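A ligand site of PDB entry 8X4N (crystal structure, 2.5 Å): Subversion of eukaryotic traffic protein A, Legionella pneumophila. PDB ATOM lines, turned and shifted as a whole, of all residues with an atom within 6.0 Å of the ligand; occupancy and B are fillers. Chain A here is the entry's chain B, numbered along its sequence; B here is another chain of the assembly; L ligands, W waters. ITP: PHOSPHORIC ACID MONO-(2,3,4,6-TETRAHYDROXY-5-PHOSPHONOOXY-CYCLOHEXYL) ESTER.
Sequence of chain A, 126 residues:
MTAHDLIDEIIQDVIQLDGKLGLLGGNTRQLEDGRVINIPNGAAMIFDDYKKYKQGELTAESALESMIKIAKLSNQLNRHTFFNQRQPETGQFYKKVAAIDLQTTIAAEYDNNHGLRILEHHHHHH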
ATOM      1  N   LYS A  20      16.334   4.400  -3.764  1.00  0.00           N
ATOM      2  CA  LYS A  20      15.210   4.681  -2.885  1.00  0.00           C
ATOM      3  C   LYS A  20      15.736   4.892  -1.472  1.00  0.00           C
ATOM      4  O   LYS A  20      15.546   4.062  -0.577  1.00  0.00           O
ATOM      5  CB  LYS A  20      14.197   3.536  -2.922  1.00  0.00           C
ATOM      6  CG  LYS A  20      13.714   3.142  -4.320  1.00  0.00           C
ATOM      7  CD  LYS A  20      13.010   4.260  -5.062  1.00  0.00           C
ATOM      8  CE  LYS A  20      12.859   3.979  -6.539  1.00  0.00           C
ATOM      9  NZ  LYS A  20      12.073   5.043  -7.203  1.00  0.00           N
ATOM     10  N   LEU A  21      16.417   6.031  -1.277  1.00  0.00           N
ATOM     11  CA  LEU A  21      17.164   6.314  -0.072  1.00  0.00           C
ATOM     12  C   LEU A  21      16.752   7.673   0.484  1.00  0.00           C
ATOM     13  O   LEU A  21      16.301   8.552  -0.264  1.00  0.00           O
ATOM     14  CB  LEU A  21      18.659   6.308  -0.400  1.00  0.00           C
ATOM     15  CG  LEU A  21      19.255   4.946  -0.723  1.00  0.00           C
ATOM     16  CD1 LEU A  21      20.655   5.104  -1.295  1.00  0.00           C
ATOM     17  CD2 LEU A  21      19.277   4.070   0.524  1.00  0.00           C
ATOM     18  N   GLY A  22      16.937   7.842   1.798  1.00  0.00           N
ATOM     19  CA  GLY A  22      16.771   9.134   2.423  1.00  0.00           C
ATOM     20  C   GLY A  22      17.905  10.081   2.020  1.00  0.00           C
ATOM     21  O   GLY A  22      18.645   9.818   1.072  1.00  0.00           O
ATOM     22  N   LEU A  23      18.033  11.176   2.782  1.00  0.00           N
ATOM     23  CA  LEU A  23      19.017  12.213   2.494  1.00  0.00           C
ATOM     24  C   LEU A  23      20.423  11.694   2.779  1.00  0.00           C
ATOM     25  O   LEU A  23      21.380  12.124   2.138  1.00  0.00           O
ATOM     26  CB  LEU A  23      18.669  13.453   3.334  1.00  0.00           C
ATOM     27  CG  LEU A  23      17.285  14.060   3.072  1.00  0.00           C
ATOM     28  CD1 LEU A  23      17.055  15.289   3.932  1.00  0.00           C
ATOM     29  CD2 LEU A  23      17.113  14.419   1.600  1.00  0.00           C
ATOM     30  N   LEU A  24      20.531  10.779   3.760  1.00  0.00           N
ATOM     31  CA  LEU A  24      21.762  10.106   4.121  1.00  0.00           C
ATOM     32  C   LEU A  24      21.617   8.600   3.935  1.00  0.00           C
ATOM     33  O   LEU A  24      20.500   8.080   3.914  1.00  0.00           O
ATOM     34  CB  LEU A  24      22.104  10.420   5.580  1.00  0.00           C
ATOM     35  CG  LEU A  24      22.755  11.780   5.820  1.00  0.00           C
ATOM     36  CD1 LEU A  24      23.099  11.958   7.287  1.00  0.00           C
ATOM     37  CD2 LEU A  24      23.991  11.943   4.948  1.00  0.00           C
ATOM     38  N   GLY A  25      22.753   7.916   3.829  1.00  0.00           N
ATOM     39  CA  GLY A  25      22.802   6.469   3.877  1.00  0.00           C
ATOM     40  C   GLY A  25      22.707   5.836   2.489  1.00  0.00           C
ATOM     41  O   GLY A  25      22.366   6.513   1.522  1.00  0.00           O
ATOM     42  N   GLY A  26      22.994   4.528   2.431  1.00  0.00           N
ATOM     43  CA  GLY A  26      22.999   3.783   1.189  1.00  0.00           C
ATOM     44  C   GLY A  26      24.089   2.722   1.185  1.00  0.00           C
ATOM     45  O   GLY A  26      25.055   2.820   1.945  1.00  0.00           O
ATOM     46  N   ASN A  27      23.928   1.725   0.330  1.00  0.00           N
ATOM     47  CA  ASN A  27      24.824   0.588   0.264  1.00  0.00           C
ATOM     48  C   ASN A  27      25.054   0.233  -1.205  1.00  0.00           C
ATOM     49  O   ASN A  27      24.111  -0.096  -1.912  1.00  0.00           O
ATOM     50  CB  ASN A  27      24.268  -0.593   1.067  1.00  0.00           C
ATOM     51  CG  ASN A  27      24.132  -0.290   2.542  1.00  0.00           C
ATOM     52  OD1 ASN A  27      25.090  -0.418   3.289  1.00  0.00           O
ATOM     53  ND2 ASN A  27      22.942   0.077   2.982  1.00  0.00           N
ATOM     54  N   ILE A  39      21.367   0.758  -2.301  1.00  0.00           N
ATOM     55  CA  ILE A  39      20.143   0.247  -1.693  1.00  0.00           C
ATOM     56  C   ILE A  39      20.191   0.386  -0.160  1.00  0.00           C
ATOM     57  O   ILE A  39      21.247   0.624   0.428  1.00  0.00           O
ATOM     58  CB  ILE A  39      19.890  -1.210  -2.128  1.00  0.00           C
ATOM     59  CG1 ILE A  39      21.084  -2.117  -1.824  1.00  0.00           C
ATOM     60  CG2 ILE A  39      19.498  -1.271  -3.598  1.00  0.00           C
ATOM     61  CD1 ILE A  39      20.805  -3.577  -2.064  1.00  0.00           C
ATOM     62  N   PRO A  40      19.020   0.241   0.513  1.00  0.00           N
ATOM     63  CA  PRO A  40      18.932   0.305   1.979  1.00  0.00           C
ATOM     64  C   PRO A  40      19.612  -0.860   2.698  1.00  0.00           C
ATOM     65  O   PRO A  40      19.926  -1.866   2.080  1.00  0.00           O
ATOM     66  CB  PRO A  40      17.418   0.244   2.250  1.00  0.00           C
ATOM     67  CG  PRO A  40      16.769   0.624   0.949  1.00  0.00           C
ATOM     68  CD  PRO A  40      17.699   0.054  -0.102  1.00  0.00           C
ATOM     69  N   ASN A  41      19.793  -0.703   4.018  1.00  0.00           N
ATOM     70  CA  ASN A  41      20.615  -1.597   4.834  1.00  0.00           C
ATOM     71  C   ASN A  41      20.085  -3.016   4.816  1.00  0.00           C
ATOM     72  O   ASN A  41      20.843  -3.955   4.563  1.00  0.00           O
ATOM     73  CB  ASN A  41      20.699  -1.154   6.292  1.00  0.00           C
ATOM     74  CG  ASN A  41      21.407   0.176   6.486  1.00  0.00           C
ATOM     75  OD1 ASN A  41      22.333   0.504   5.748  1.00  0.00           O
ATOM     76  ND2 ASN A  41      20.957   0.951   7.470  1.00  0.00           N
ATOM     77  N   GLY A  42      18.787  -3.169   5.108  1.00  0.00           N
ATOM     78  CA  GLY A  42      18.129  -4.466   5.121  1.00  0.00           C
ATOM     79  C   GLY A  42      18.224  -5.179   3.780  1.00  0.00           C
ATOM     80  O   GLY A  42      18.560  -6.357   3.712  1.00  0.00           O
ATOM     81  N   ALA A  43      17.937  -4.435   2.701  1.00  0.00           N
ATOM     82  CA  ALA A  43      17.956  -4.969   1.353  1.00  0.00           C
ATOM     83  C   ALA A  43      19.369  -5.381   0.932  1.00  0.00           C
ATOM     84  O   ALA A  43      19.535  -6.275   0.117  1.00  0.00           O
ATOM     85  CB  ALA A  43      17.386  -3.955   0.386  1.00  0.00           C
ATOM     86  N   SER A  74      13.919  -5.909  10.023  1.00  0.00           N
ATOM     87  CA  SER A  74      13.874  -4.612   9.356  1.00  0.00           C
ATOM     88  C   SER A  74      12.480  -3.997   9.504  1.00  0.00           C
ATOM     89  O   SER A  74      12.339  -2.795   9.663  1.00  0.00           O
ATOM     90  CB  SER A  74      14.293  -4.722   7.912  1.00  0.00           C
ATOM     91  OG  SER A  74      15.667  -5.032   7.821  1.00  0.00           O
ATOM     92  N   LEU A  77      12.016  -2.169  12.768  1.00  0.00           N
ATOM     93  CA  LEU A  77      12.834  -0.981  12.964  1.00  0.00           C
ATOM     94  C   LEU A  77      12.176   0.231  12.313  1.00  0.00           C
ATOM     95  O   LEU A  77      11.991   0.255  11.099  1.00  0.00           O
ATOM     96  CB  LEU A  77      14.216  -1.250  12.366  1.00  0.00           C
ATOM     97  CG  LEU A  77      15.279  -0.191  12.665  1.00  0.00           C
ATOM     98  CD1 LEU A  77      15.923  -0.425  14.021  1.00  0.00           C
ATOM     99  CD2 LEU A  77      16.338  -0.167  11.572  1.00  0.00           C
ATOM    100  N   HIS A  80      14.024   5.754  12.228  1.00  0.00           N
ATOM    101  CA  HIS A  80      14.576   6.629  11.203  1.00  0.00           C
ATOM    102  C   HIS A  80      14.295   8.088  11.547  1.00  0.00           C
ATOM    103  O   HIS A  80      13.235   8.397  12.093  1.00  0.00           O
ATOM    104  CB  HIS A  80      14.006   6.266   9.823  1.00  0.00           C
ATOM    105  CG  HIS A  80      14.317   4.871   9.413  1.00  0.00           C
ATOM    106  ND1 HIS A  80      13.594   3.796   9.859  1.00  0.00           N
ATOM    107  CD2 HIS A  80      15.267   4.374   8.600  1.00  0.00           C
ATOM    108  CE1 HIS A  80      14.087   2.683   9.324  1.00  0.00           C
ATOM    109  NE2 HIS A  80      15.113   3.014   8.562  1.00  0.00           N
ATOM    110  N   PHE A  83      16.493  12.717   8.221  1.00  0.00           N
ATOM    111  CA  PHE A  83      17.676  12.737   7.366  1.00  0.00           C
ATOM    112  C   PHE A  83      17.952  11.376   6.724  1.00  0.00           C
ATOM    113  O   PHE A  83      18.778  11.320   5.820  1.00  0.00           O
ATOM    114  CB  PHE A  83      18.907  13.143   8.181  1.00  0.00           C
ATOM    115  CG  PHE A  83      18.953  14.583   8.657  1.00  0.00           C
ATOM    116  CD1 PHE A  83      18.016  15.520   8.253  1.00  0.00           C
ATOM    117  CD2 PHE A  83      19.973  14.991   9.502  1.00  0.00           C
ATOM    118  CE1 PHE A  83      18.087  16.827   8.692  1.00  0.00           C
ATOM    119  CE2 PHE A  83      20.038  16.310   9.945  1.00  0.00           C
ATOM    120  CZ  PHE A  83      19.100  17.225   9.530  1.00  0.00           C
ATOM    121  N   ASN A  84      17.308  10.304   7.213  1.00  0.00           N
ATOM    122  CA  ASN A  84      17.509   8.943   6.723  1.00  0.00           C
ATOM    123  C   ASN A  84      16.199   8.157   6.713  1.00  0.00           C
ATOM    124  O   ASN A  84      16.149   7.020   7.174  1.00  0.00           O
ATOM    125  CB  ASN A  84      18.561   8.180   7.540  1.00  0.00           C
ATOM    126  CG  ASN A  84      18.251   8.028   9.019  1.00  0.00           C
ATOM    127  OD1 ASN A  84      17.482   8.787   9.591  1.00  0.00           O
ATOM    128  ND2 ASN A  84      18.896   7.065   9.654  1.00  0.00           N
ATOM    129  N   GLN A  85      15.147   8.754   6.140  1.00  0.00           N
ATOM    130  CA  GLN A  85      13.837   8.130   6.095  1.00  0.00           C
ATOM    131  C   GLN A  85      13.867   6.887   5.206  1.00  0.00           C
ATOM    132  O   GLN A  85      14.469   6.902   4.130  1.00  0.00           O
ATOM    133  CB  GLN A  85      12.781   9.094   5.546  1.00  0.00           C
ATOM    134  CG  GLN A  85      12.508  10.302   6.424  1.00  0.00           C
ATOM    135  CD  GLN A  85      11.742  11.354   5.654  1.00  0.00           C
ATOM    136  OE1 GLN A  85      10.751  11.059   4.991  1.00  0.00           O
ATOM    137  NE2 GLN A  85      12.216  12.592   5.720  1.00  0.00           N
ATOM    138  N   ARG A  86      13.167   5.836   5.664  1.00  0.00           N
ATOM    139  CA  ARG A  86      12.841   4.690   4.837  1.00  0.00           C
ATOM    140  C   ARG A  86      11.708   5.051   3.890  1.00  0.00           C
ATOM    141  O   ARG A  86      10.671   5.554   4.319  1.00  0.00           O
ATOM    142  CB  ARG A  86      12.396   3.502   5.693  1.00  0.00           C
ATOM    143  CG  ARG A  86      12.019   2.266   4.875  1.00  0.00           C
ATOM    144  CD  ARG A  86      11.589   1.125   5.765  1.00  0.00           C
ATOM    145  NE  ARG A  86      12.687   0.687   6.612  1.00  0.00           N
ATOM    146  CZ  ARG A  86      12.558  -0.138   7.638  1.00  0.00           C
ATOM    147  NH1 ARG A  86      11.356  -0.561   7.991  1.00  0.00           N
ATOM    148  NH2 ARG A  86      13.626  -0.532   8.307  1.00  0.00           N
ATOM    149  N   GLN A  87      11.916   4.757   2.604  1.00  0.00           N
ATOM    150  CA  GLN A  87      10.934   5.077   1.572  1.00  0.00           C
ATOM    151  C   GLN A  87       9.783   4.066   1.662  1.00  0.00           C
ATOM    152  O   GLN A  87       9.964   2.970   2.199  1.00  0.00           O
ATOM    153  CB  GLN A  87      11.607   5.063   0.198  1.00  0.00           C
ATOM    154  CG  GLN A  87      12.812   5.986   0.107  1.00  0.00           C
ATOM    155  CD  GLN A  87      12.467   7.430   0.393  1.00  0.00           C
ATOM    156  OE1 GLN A  87      11.697   8.038  -0.336  1.00  0.00           O
ATOM    157  NE2 GLN A  87      13.037   7.987   1.444  1.00  0.00           N
ATOM    158  N   THR A  90      10.417   0.703   0.000  1.00  0.00           N
ATOM    159  CA  THR A  90      11.259  -0.169   0.806  1.00  0.00           C
ATOM    160  C   THR A  90      10.445  -0.821   1.913  1.00  0.00           C
ATOM    161  O   THR A  90      10.711  -1.959   2.288  1.00  0.00           O
ATOM    162  CB  THR A  90      12.459   0.619   1.355  1.00  0.00           C
ATOM    163  OG1 THR A  90      13.214   1.113   0.248  1.00  0.00           O
ATOM    164  CG2 THR A  90      13.354  -0.211   2.248  1.00  0.00           C
ATOM    165  N   TYR A  94       9.916  -5.035   2.640  1.00  0.00           N
ATOM    166  CA  TYR A  94      10.220  -5.752   3.868  1.00  0.00           C
ATOM    167  C   TYR A  94       8.964  -6.455   4.395  1.00  0.00           C
ATOM    168  O   TYR A  94       9.064  -7.515   4.993  1.00  0.00           O
ATOM    169  CB  TYR A  94      10.804  -4.838   4.951  1.00  0.00           C
ATOM    170  CG  TYR A  94      12.170  -4.254   4.655  1.00  0.00           C
ATOM    171  CD1 TYR A  94      13.164  -4.990   4.029  1.00  0.00           C
ATOM    172  CD2 TYR A  94      12.495  -2.974   5.083  1.00  0.00           C
ATOM    173  CE1 TYR A  94      14.426  -4.448   3.790  1.00  0.00           C
ATOM    174  CE2 TYR A  94      13.742  -2.425   4.850  1.00  0.00           C
ATOM    175  CZ  TYR A  94      14.714  -3.156   4.195  1.00  0.00           C
ATOM    176  OH  TYR A  94      15.947  -2.605   3.959  1.00  0.00           O
ATOM    177  N   MET B  45      20.798  10.684  15.326  1.00  0.00           N
ATOM    178  CA  MET B  45      21.652   9.762  14.579  1.00  0.00           C
ATOM    179  C   MET B  45      22.991   9.605  15.298  1.00  0.00           C
ATOM    180  O   MET B  45      23.619   8.540  15.238  1.00  0.00           O
ATOM    181  CB  MET B  45      21.900  10.294  13.167  1.00  0.00           C
ATOM    182  CG  MET B  45      20.688  10.159  12.270  1.00  0.00           C
ATOM    183  SD  MET B  45      21.005  10.869  10.640  1.00  0.00           S
ATOM    184  CE  MET B  45      21.849   9.502   9.853  1.00  0.00           C
ATOM    185  N   LYS B  52      25.285   1.792  18.952  1.00  0.00           N
ATOM    186  CA  LYS B  52      26.057   0.814  18.215  1.00  0.00           C
ATOM    187  C   LYS B  52      27.422   0.587  18.861  1.00  0.00           C
ATOM    188  O   LYS B  52      27.911  -0.536  18.874  1.00  0.00           O
ATOM    189  CB  LYS B  52      26.207   1.252  16.751  1.00  0.00           C
ATOM    190  CG  LYS B  52      24.948   1.080  15.915  1.00  0.00           C
ATOM    191  CD  LYS B  52      25.038   1.689  14.544  1.00  0.00           C
ATOM    192  CE  LYS B  52      23.729   1.589  13.789  1.00  0.00           C
ATOM    193  NZ  LYS B  52      23.839   2.233  12.446  1.00  0.00           N
HETATM  194  C1  ITP L   1      18.996   4.696   5.667  1.00  0.00           C
HETATM  195  O1  ITP L   1      20.377   5.173   5.792  1.00  0.00           O
HETATM  196  C2  ITP L   1      19.014   3.175   5.637  1.00  0.00           C
HETATM  197  O2  ITP L   1      19.849   2.699   4.579  1.00  0.00           O
HETATM  198  C3  ITP L   1      17.582   2.650   5.475  1.00  0.00           C
HETATM  199  O3  ITP L   1      17.616   1.190   5.414  1.00  0.00           O
HETATM  200  C4  ITP L   1      16.943   3.201   4.207  1.00  0.00           C
HETATM  201  O4  ITP L   1      15.600   2.738   4.079  1.00  0.00           O
HETATM  202  C5  ITP L   1      16.961   4.718   4.231  1.00  0.00           C
HETATM  203  O5  ITP L   1      16.366   5.225   3.039  1.00  0.00           O
HETATM  204  C6  ITP L   1      18.375   5.247   4.377  1.00  0.00           C
HETATM  205  O6  ITP L   1      18.362   6.676   4.390  1.00  0.00           O
HETATM  206  P1  ITP L   1      21.229   5.174   7.180  1.00  0.00           P
HETATM  207  OP1 ITP L   1      21.926   6.529   7.232  1.00  0.00           O
HETATM  208  OP2 ITP L   1      20.288   4.973   8.364  1.00  0.00           O
HETATM  209  OP3 ITP L   1      22.195   4.025   7.014  1.00  0.00           O
HETATM  210  P3  ITP L   1      16.458   0.291   6.110  1.00  0.00           P
HETATM  211  O10 ITP L   1      16.303   0.765   7.544  1.00  0.00           O
HETATM  212  O11 ITP L   1      16.914  -1.145   6.030  1.00  0.00           O
HETATM  213  O12 ITP L   1      15.217   0.547   5.301  1.00  0.00           O
HETATM  214  O   HOH W   1      17.321  -2.819   8.376  1.00  0.00           O
HETATM  215  O   HOH W   2      18.555   0.458   8.578  1.00  0.00           O
HETATM  216  O   HOH W   3      19.089   2.673   9.798  1.00  0.00           O
HETATM  217  O   HOH W   4      22.509   2.797   4.963  1.00  0.00           O
HETATM  218  O   HOH W   5      14.458   3.348   1.825  1.00  0.00           O
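NE of Arg 86 is in salt-bridge range of O12 of the ligand, at 2.9 Å. OH of Tyr 94 lies within hydrogen-bond range of O11 of the ligand, at 2.7 Å. N of Gly 22 lies within hydrogen-bond range of O5 of the ligand (3.0 Å). N of Asn 41 sits at hydrogen-bond distance from O3 of the ligand (3.2 Å). ND2 of Asn 41 lies within hydrogen-bond range of OP3 of the ligand, at 3.3 Å. A ring nitrogen (NE2) of His 80 lies within hydrogen-bond range of an oxygen (O10) of the ligand (2.7 Å). The side-chain amide nitrogen of Asn 84 is in hydrogen-bond range of an oxygen (OP2) of the ligand, at 2.8 Å. The backbone carbonyl oxygen of Gln 85 lies within hydrogen-bond range of an oxygen (O5) of the ligand. O of Leu 24 sits at hydrogen-bond distance from O6 of the ligand (2.6 Å). The backbone NH (N) of Gly 42 sits at hydrogen-bond distance from an oxygen (O11) of the ligand (2.9 Å).
The backbone NH (N) of Leu 24 sits at hydrogen-bond distance from the backbone carbonyl oxygen (O) of Phe 83 (2.8 Å). NE2 of Gln 87 is in hydrogen-bond range of O of Gln 85 (3.2 Å). O of Leu 77 is in hydrogen-bond range of NH1 of Arg 86, 3.3 Å away. OD1 of Asn 41 lies within hydrogen-bond range of ND2 of Asn 27 (2.9 Å). OH of Tyr 94 lies close to N of Gly 42 (3.1 Å). The backbone carbonyl oxygen (O) of Ser 74 lies within hydrogen-bond range of the guanidinium group (NH2) of Arg 86. N of Ala 43 sits at hydrogen-bond distance from OH of Tyr 94, at 3.0 Å.
Lys 20 touches the ligand (O to O5, 3.9 Å). CA of Leu 21 touches O5 of the ligand, at 3.4 Å. Gly 25 touches the ligand (CA to O1, 3.4 Å). CB of Pro 40 touches O3 of the ligand, at 3.3 Å. Thr 90 touches the ligand. CE of Met 45 of chain B touches OP1 of the ligand, at 3.96 Å. Hydrophobic or aromatic side chains that line the ligand: Pro 40, His 80, Tyr 94 and Met 45 of chain B. Within 4 Å of the ligand: Lys 20, Leu 21, Gly 22, Leu 24, Gly 25, Pro 40, Asn 41, Gly 42, His 80, Asn 84, Gln 85, Arg 86, Thr 90, Tyr 94 and Met 45 of chain B.
Water W4 lies within hydrogen-bond range of an oxygen (OP3) of the ligand (2.4 Å), the side-chain amide oxygen of Asn 41 (2.4 Å), the backbone NH of Gly 26 (3.1 Å) and the side-chain amide nitrogen of Asn 27 (3.4 Å). Water W2 bridges O10 of the ligand (2.5 Å) and ND2 of Asn 41 (2.7 Å). Water W5 lies within hydrogen-bond range of an oxygen (O4) of the ligand (2.6 Å), the backbone carbonyl oxygen (O) of Lys 20 (2.7 Å), the side-chain hydroxyl (OG1) of Thr 90 (3.0 Å) and the backbone NH (N) of Gln 87 (3.0 Å). Water W1 bridges OG of Ser 74 and O11 of the ligand. Water W3 bridges OP2 of the ligand and ND2 of Asn 41.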
